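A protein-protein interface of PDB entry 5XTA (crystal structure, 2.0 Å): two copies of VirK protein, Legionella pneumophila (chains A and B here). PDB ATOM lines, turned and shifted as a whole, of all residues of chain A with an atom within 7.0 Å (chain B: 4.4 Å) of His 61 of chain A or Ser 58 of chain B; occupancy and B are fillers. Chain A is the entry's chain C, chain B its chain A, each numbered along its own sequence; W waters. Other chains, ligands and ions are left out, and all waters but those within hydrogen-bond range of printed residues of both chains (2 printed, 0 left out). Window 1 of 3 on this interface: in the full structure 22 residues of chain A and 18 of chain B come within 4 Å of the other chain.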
ATOM      1  N   VAL A  42      -6.695 -18.895  11.056  1.00  0.00           N
ATOM      2  CA  VAL A  42      -6.382 -17.470  11.100  1.00  0.00           C
ATOM      3  C   VAL A  42      -6.664 -16.931  12.495  1.00  0.00           C
ATOM      4  O   VAL A  42      -7.735 -17.150  13.028  1.00  0.00           O
ATOM      5  CB  VAL A  42      -7.238 -16.651  10.087  1.00  0.00           C
ATOM      6  CG1 VAL A  42      -6.940 -15.153  10.176  1.00  0.00           C
ATOM      7  CG2 VAL A  42      -6.969 -17.096   8.663  1.00  0.00           C
ATOM      8  N   ASP A  59      -9.030 -10.216   8.090  1.00  0.00           N
ATOM      9  CA  ASP A  59      -7.579 -10.413   7.927  1.00  0.00           C
ATOM     10  C   ASP A  59      -7.179 -10.041   6.539  1.00  0.00           C
ATOM     11  O   ASP A  59      -7.782 -10.501   5.560  1.00  0.00           O
ATOM     12  CB  ASP A  59      -7.227 -11.887   8.163  1.00  0.00           C
ATOM     13  CG  ASP A  59      -5.695 -12.167   8.141  1.00  0.00           C
ATOM     14  OD1 ASP A  59      -4.971 -11.603   8.970  1.00  0.00           O
ATOM     15  OD2 ASP A  59      -5.236 -12.987   7.307  1.00  0.00           O
ATOM     16  N   ARG A  60      -6.170  -9.211   6.440  1.00  0.00           N
ATOM     17  CA  ARG A  60      -5.591  -8.839   5.168  1.00  0.00           C
ATOM     18  C   ARG A  60      -4.305  -9.626   5.011  1.00  0.00           C
ATOM     19  O   ARG A  60      -3.321  -9.357   5.727  1.00  0.00           O
ATOM     20  CB  ARG A  60      -5.340  -7.319   5.125  1.00  0.00           C
ATOM     21  CG  ARG A  60      -4.632  -6.920   3.832  1.00  0.00           C
ATOM     22  CD  ARG A  60      -4.198  -5.486   3.777  1.00  0.00           C
ATOM     23  NE  ARG A  60      -3.046  -5.271   4.633  1.00  0.00           N
ATOM     24  CZ  ARG A  60      -2.152  -4.292   4.529  1.00  0.00           C
ATOM     25  NH1 ARG A  60      -2.160  -3.428   3.534  1.00  0.00           N
ATOM     26  NH2 ARG A  60      -1.183  -4.231   5.408  1.00  0.00           N
ATOM     27  N   HIS A  61      -4.317 -10.617   4.107  1.00  0.00           N
ATOM     28  CA  HIS A  61      -3.234 -11.558   3.980  1.00  0.00           C
ATOM     29  C   HIS A  61      -2.434 -11.357   2.673  1.00  0.00           C
ATOM     30  O   HIS A  61      -2.949 -11.553   1.585  1.00  0.00           O
ATOM     31  CB  HIS A  61      -3.805 -12.956   4.053  1.00  0.00           C
ATOM     32  CG  HIS A  61      -2.769 -14.011   3.913  1.00  0.00           C
ATOM     33  ND1 HIS A  61      -1.864 -14.279   4.914  1.00  0.00           N
ATOM     34  CD2 HIS A  61      -2.429 -14.800   2.867  1.00  0.00           C
ATOM     35  CE1 HIS A  61      -1.030 -15.217   4.502  1.00  0.00           C
ATOM     36  NE2 HIS A  61      -1.359 -15.561   3.269  1.00  0.00           N
ATOM     37  N   PHE A  62      -1.167 -11.000   2.791  1.00  0.00           N
ATOM     38  CA  PHE A  62      -0.331 -10.784   1.608  1.00  0.00           C
ATOM     39  C   PHE A  62       0.102 -12.118   1.007  1.00  0.00           C
ATOM     40  O   PHE A  62       0.445 -13.046   1.746  1.00  0.00           O
ATOM     41  CB  PHE A  62       0.898  -9.991   1.972  1.00  0.00           C
ATOM     42  CG  PHE A  62       1.777  -9.673   0.807  1.00  0.00           C
ATOM     43  CD1 PHE A  62       1.513  -8.551   0.020  1.00  0.00           C
ATOM     44  CD2 PHE A  62       2.887 -10.447   0.531  1.00  0.00           C
ATOM     45  CE1 PHE A  62       2.325  -8.213  -1.045  1.00  0.00           C
ATOM     46  CE2 PHE A  62       3.712 -10.129  -0.533  1.00  0.00           C
ATOM     47  CZ  PHE A  62       3.428  -9.021  -1.330  1.00  0.00           C
ATOM     48  N   THR A  63       0.054 -12.223  -0.310  1.00  0.00           N
ATOM     49  CA  THR A  63       0.420 -13.456  -0.987  1.00  0.00           C
ATOM     50  C   THR A  63       0.985 -13.182  -2.387  1.00  0.00           C
ATOM     51  O   THR A  63       0.679 -12.162  -3.032  1.00  0.00           O
ATOM     52  CB  THR A  63      -0.792 -14.432  -1.040  1.00  0.00           C
ATOM     53  OG1 THR A  63      -0.376 -15.760  -1.431  1.00  0.00           O
ATOM     54  CG2 THR A  63      -1.910 -13.914  -1.983  1.00  0.00           C
ATOM     55  N   LEU A  64       1.818 -14.111  -2.841  1.00  0.00           N
ATOM     56  CA  LEU A  64       2.175 -14.198  -4.259  1.00  0.00           C
ATOM     57  C   LEU A  64       1.530 -15.443  -4.886  1.00  0.00           C
ATOM     58  O   LEU A  64       1.789 -15.746  -6.043  1.00  0.00           O
ATOM     59  CB  LEU A  64       3.689 -14.299  -4.424  1.00  0.00           C
ATOM     60  CG  LEU A  64       4.634 -13.106  -4.353  1.00  0.00           C
ATOM     61  CD1 LEU A  64       4.255 -12.170  -3.248  1.00  0.00           C
ATOM     62  CD2 LEU A  64       6.074 -13.570  -4.202  1.00  0.00           C
ATOM     63  N   ASP A  65       0.720 -16.176  -4.128  1.00  0.00           N
ATOM     64  CA  ASP A  65       0.295 -17.519  -4.530  1.00  0.00           C
ATOM     65  C   ASP A  65      -1.184 -17.568  -4.914  1.00  0.00           C
ATOM     66  O   ASP A  65      -1.747 -18.663  -5.052  1.00  0.00           O
ATOM     67  CB  ASP A  65       0.619 -18.512  -3.393  1.00  0.00           C
ATOM     68  CG  ASP A  65       2.056 -18.332  -2.840  1.00  0.00           C
ATOM     69  OD1 ASP A  65       3.028 -18.758  -3.500  1.00  0.00           O
ATOM     70  OD2 ASP A  65       2.222 -17.751  -1.743  1.00  0.00           O
ATOM     71  N   MET A  74      -0.335  -9.470  -4.013  1.00  0.00           N
ATOM     72  CA  MET A  74      -1.778  -9.335  -3.793  1.00  0.00           C
ATOM     73  C   MET A  74      -2.105  -9.437  -2.332  1.00  0.00           C
ATOM     74  O   MET A  74      -1.336 -10.035  -1.569  1.00  0.00           O
ATOM     75  CB  MET A  74      -2.514 -10.466  -4.502  1.00  0.00           C
ATOM     76  CG  MET A  74      -2.683 -10.264  -6.003  1.00  0.00           C
ATOM     77  SD  MET A  74      -3.411 -11.953  -6.670  1.00  0.00           S
ATOM     78  CE  MET A  74      -1.797 -13.033  -6.408  1.00  0.00           C
ATOM     79  N   PHE A  75      -3.243  -8.858  -1.943  1.00  0.00           N
ATOM     80  CA  PHE A  75      -3.816  -9.057  -0.599  1.00  0.00           C
ATOM     81  C   PHE A  75      -5.086  -9.849  -0.763  1.00  0.00           C
ATOM     82  O   PHE A  75      -5.940  -9.480  -1.549  1.00  0.00           O
ATOM     83  CB  PHE A  75      -4.170  -7.752   0.098  1.00  0.00           C
ATOM     84  CG  PHE A  75      -2.982  -6.928   0.509  1.00  0.00           C
ATOM     85  CD1 PHE A  75      -2.085  -7.385   1.482  1.00  0.00           C
ATOM     86  CD2 PHE A  75      -2.756  -5.713  -0.080  1.00  0.00           C
ATOM     87  CE1 PHE A  75      -0.995  -6.622   1.851  1.00  0.00           C
ATOM     88  CE2 PHE A  75      -1.662  -4.944   0.286  1.00  0.00           C
ATOM     89  CZ  PHE A  75      -0.759  -5.415   1.240  1.00  0.00           C
ATOM     90  N   ASP A  76      -5.163 -10.971  -0.059  1.00  0.00           N
ATOM     91  CA  ASP A  76      -6.409 -11.714   0.112  1.00  0.00           C
ATOM     92  C   ASP A  76      -7.051 -11.182   1.372  1.00  0.00           C
ATOM     93  O   ASP A  76      -6.572 -11.470   2.481  1.00  0.00           O
ATOM     94  CB  ASP A  76      -6.131 -13.216   0.263  1.00  0.00           C
ATOM     95  CG  ASP A  76      -5.841 -13.890  -1.055  1.00  0.00           C
ATOM     96  OD1 ASP A  76      -5.856 -13.216  -2.099  1.00  0.00           O
ATOM     97  OD2 ASP A  76      -5.612 -15.116  -1.048  1.00  0.00           O
ATOM     98  N   TYR A  77      -8.088 -10.364   1.209  1.00  0.00           N
ATOM     99  CA  TYR A  77      -8.784  -9.803   2.348  1.00  0.00           C
ATOM    100  C   TYR A  77      -9.991 -10.689   2.677  1.00  0.00           C
ATOM    101  O   TYR A  77     -10.922 -10.865   1.868  1.00  0.00           O
ATOM    102  CB  TYR A  77      -9.172  -8.367   2.073  1.00  0.00           C
ATOM    103  CG  TYR A  77     -10.083  -7.771   3.118  1.00  0.00           C
ATOM    104  CD1 TYR A  77      -9.582  -7.347   4.339  1.00  0.00           C
ATOM    105  CD2 TYR A  77     -11.456  -7.674   2.911  1.00  0.00           C
ATOM    106  CE1 TYR A  77     -10.400  -6.790   5.301  1.00  0.00           C
ATOM    107  CE2 TYR A  77     -12.294  -7.144   3.876  1.00  0.00           C
ATOM    108  CZ  TYR A  77     -11.760  -6.675   5.079  1.00  0.00           C
ATOM    109  OH  TYR A  77     -12.552  -6.120   6.082  1.00  0.00           O
ATOM    110  N   SER A  78      -9.985 -11.237   3.875  1.00  0.00           N
ATOM    111  CA  SER A  78     -11.042 -12.137   4.324  1.00  0.00           C
ATOM    112  C   SER A  78     -11.819 -11.482   5.465  1.00  0.00           C
ATOM    113  O   SER A  78     -11.225 -11.054   6.443  1.00  0.00           O
ATOM    114  CB  SER A  78     -10.472 -13.456   4.793  1.00  0.00           C
ATOM    115  OG  SER A  78      -9.956 -14.153   3.691  1.00  0.00           O
ATOM    116  N   PRO B  44       3.597 -16.939  11.974  1.00  0.00           N
ATOM    117  CA  PRO B  44       2.547 -16.326  11.166  1.00  0.00           C
ATOM    118  C   PRO B  44       1.216 -16.383  11.852  1.00  0.00           C
ATOM    119  O   PRO B  44       0.975 -17.279  12.651  1.00  0.00           O
ATOM    120  CB  PRO B  44       2.542 -17.155   9.894  1.00  0.00           C
ATOM    121  CG  PRO B  44       3.508 -18.285  10.100  1.00  0.00           C
ATOM    122  CD  PRO B  44       3.952 -18.295  11.524  1.00  0.00           C
ATOM    123  N   ALA B  57       2.384 -21.727   4.867  1.00  0.00           N
ATOM    124  CA  ALA B  57       2.208 -20.442   5.548  1.00  0.00           C
ATOM    125  C   ALA B  57       3.140 -19.471   4.931  1.00  0.00           C
ATOM    126  O   ALA B  57       4.009 -19.862   4.188  1.00  0.00           O
ATOM    127  CB  ALA B  57       2.506 -20.554   7.032  1.00  0.00           C
ATOM    128  N   SER B  58       2.959 -18.202   5.229  1.00  0.00           N
ATOM    129  CA  SER B  58       3.882 -17.168   4.709  1.00  0.00           C
ATOM    130  C   SER B  58       4.011 -15.991   5.648  1.00  0.00           C
ATOM    131  O   SER B  58       3.194 -15.827   6.578  1.00  0.00           O
ATOM    132  CB  SER B  58       3.402 -16.689   3.334  1.00  0.00           C
ATOM    133  OG  SER B  58       2.176 -15.967   3.396  1.00  0.00           O
ATOM    134  N   ASP B  59       5.033 -15.173   5.413  1.00  0.00           N
ATOM    135  CA  ASP B  59       5.306 -13.992   6.248  1.00  0.00           C
ATOM    136  C   ASP B  59       5.923 -12.935   5.355  1.00  0.00           C
ATOM    137  O   ASP B  59       6.876 -13.210   4.630  1.00  0.00           O
ATOM    138  CB  ASP B  59       6.268 -14.314   7.444  1.00  0.00           C
ATOM    139  CG  ASP B  59       6.598 -13.080   8.314  1.00  0.00           C
ATOM    140  OD1 ASP B  59       5.716 -12.501   8.945  1.00  0.00           O
ATOM    141  OD2 ASP B  59       7.739 -12.623   8.399  1.00  0.00           O
ATOM    142  N   TYR B  77       9.499 -11.513   1.583  1.00  0.00           N
ATOM    143  CA  TYR B  77       8.381 -12.411   1.635  1.00  0.00           C
ATOM    144  C   TYR B  77       8.858 -13.873   1.622  1.00  0.00           C
ATOM    145  O   TYR B  77       9.470 -14.344   0.633  1.00  0.00           O
ATOM    146  CB  TYR B  77       7.467 -12.150   0.449  1.00  0.00           C
ATOM    147  CG  TYR B  77       6.346 -13.137   0.300  1.00  0.00           C
ATOM    148  CD1 TYR B  77       5.243 -13.090   1.134  1.00  0.00           C
ATOM    149  CD2 TYR B  77       6.388 -14.138  -0.667  1.00  0.00           C
ATOM    150  CE1 TYR B  77       4.187 -13.984   0.984  1.00  0.00           C
ATOM    151  CE2 TYR B  77       5.352 -15.052  -0.801  1.00  0.00           C
ATOM    152  CZ  TYR B  77       4.253 -14.972   0.033  1.00  0.00           C
ATOM    153  OH  TYR B  77       3.226 -15.857  -0.077  1.00  0.00           O
ATOM    154  N   SER B  78       8.546 -14.591   2.695  1.00  0.00           N
ATOM    155  CA  SER B  78       8.910 -15.980   2.841  1.00  0.00           C
ATOM    156  C   SER B  78       7.678 -16.850   2.773  1.00  0.00           C
ATOM    157  O   SER B  78       6.722 -16.614   3.494  1.00  0.00           O
ATOM    158  CB  SER B  78       9.609 -16.171   4.158  1.00  0.00           C
ATOM    159  OG  SER B  78      10.824 -15.462   4.127  1.00  0.00           O
ATOM    160  N   LYS B  79       7.722 -17.847   1.885  1.00  0.00           N
ATOM    161  CA  LYS B  79       6.702 -18.873   1.738  1.00  0.00           C
ATOM    162  C   LYS B  79       7.234 -20.217   2.297  1.00  0.00           C
ATOM    163  O   LYS B  79       8.285 -20.687   1.892  1.00  0.00           O
ATOM    164  CB  LYS B  79       6.346 -18.960   0.254  1.00  0.00           C
ATOM    165  CG  LYS B  79       5.409 -20.085  -0.148  1.00  0.00           C
ATOM    166  CD  LYS B  79       4.018 -19.846   0.367  1.00  0.00           C
ATOM    167  CE  LYS B  79       3.101 -20.954  -0.132  1.00  0.00           C
ATOM    168  NZ  LYS B  79       1.795 -20.887   0.544  1.00  0.00           N
ATOM    169  N   PHE B  80       6.536 -20.758   3.284  1.00  0.00           N
ATOM    170  CA  PHE B  80       6.955 -21.960   4.012  1.00  0.00           C
ATOM    171  C   PHE B  80       6.071 -23.087   3.524  1.00  0.00           C
ATOM    172  O   PHE B  80       4.857 -22.915   3.432  1.00  0.00           O
ATOM    173  CB  PHE B  80       6.714 -21.788   5.511  1.00  0.00           C
ATOM    174  CG  PHE B  80       7.504 -20.682   6.132  1.00  0.00           C
ATOM    175  CD1 PHE B  80       8.745 -20.930   6.677  1.00  0.00           C
ATOM    176  CD2 PHE B  80       7.007 -19.385   6.179  1.00  0.00           C
ATOM    177  CE1 PHE B  80       9.487 -19.914   7.253  1.00  0.00           C
ATOM    178  CE2 PHE B  80       7.745 -18.370   6.762  1.00  0.00           C
ATOM    179  CZ  PHE B  80       8.990 -18.641   7.298  1.00  0.00           C
HETATM  180  O   HOH W   1       0.565 -16.541   0.956  1.00  0.00           O
HETATM  181  O   HOH W   2       2.030 -13.478   3.986  1.00  0.00           O
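OD2 of Asp 65 of chain A sits at hydrogen-bond distance from OH of Tyr 77 of chain B.
OD2 of Asp 65 of chain A lies within salt-bridge range of NZ of Lys 79 of chain B.
The side-chain hydroxyl of Thr 63 of chain A sits at hydrogen-bond distance from the backbone NH of Asp 65 of chain A (2.9 Å).
The backbone NH (N) of Thr 63 of chain A is in hydrogen-bond range of the backbone carbonyl oxygen (O) of Met 74 of chain A (2.9 Å).
The backbone NH (N) of Asp 76 of chain A is in hydrogen-bond range of the backbone carbonyl oxygen (O) of His 61 of chain A (2.8 Å).
Among the printed residues, pairs that only touch across the chains: His 61 of chain A with Ser 58 of chain B, Phe 62 of chain A with Ser 58 of chain B, Phe 62 of chain A with Tyr 77 of chain B, Thr 63 of chain A with Tyr 77 of chain B and Leu 64 of chain A with Tyr 77 of chain B.
Of the printed residues of chain B, His 61 of chain A touches Ser 58 (3.5 Å).
Printed residues of chain B within 4 Å of Phe 62 of chain A: Ser 58 (3.8 Å) and Tyr 77 (3.6 Å).
Printed residues of chain B within 4 Å of Asp 65 of chain A: Tyr 77 and Lys 79.
Ser 78 of chain A touches none of the printed residues of chain B.
Of chain A, only His 61 (3.5 Å) and Phe 62 (3.8 Å) come within 4 Å of Ser 58 of chain B.
Printed residues of chain A within 4 Å of Tyr 77 of chain B: Phe 62, Thr 63, Leu 64 and Asp 65.
The nearest printed residue of chain B that does not touch His 61 of chain A is Tyr 77 of chain B (5.7 Å).
The nearest printed residue of chain B that does not touch Leu 64 of chain A is Ser 58 of chain B (6.5 Å).
Printed residues of chain B that touch a printed residue of chain A: Ser 58, Tyr 77 and Lys 79.
Hydrophobic or aromatic side chains of chain B that line the printed part of chain A: Tyr 77.
Of the 13 printed residues of chain A, 5 touch a printed residue of chain B.
Along chain A the printed residues that touch a printed residue of chain B span positions 61 to 65.
Among the printed residues, Asp or Glu carboxylates within 4 Å of a Lys or Arg side-chain nitrogen of the other chain: Asp 65 of chain A with Lys 79 of chain B.
Positions printed for both chains: 59, 77 and 78.
Of the 7 pairs that touch across the chains among the printed residues, none has its exchanged pair printed and touching as well.
Water W2 bridges the side-chain hydroxyl (OG) of Ser 58 of chain B (2.6 Å) and the backbone carbonyl oxygen (O) of Phe 62 of chain A (2.8 Å).
Water W1 lies within hydrogen-bond range of OG1 of Thr 63 of chain A (2.7 Å), OH of Tyr 77 of chain B (2.9 Å), OG of Ser 58 of chain B (3.0 Å), NE2 of His 61 of chain A (3.2 Å) and OD2 of Asp 65 of chain A (3.4 Å).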
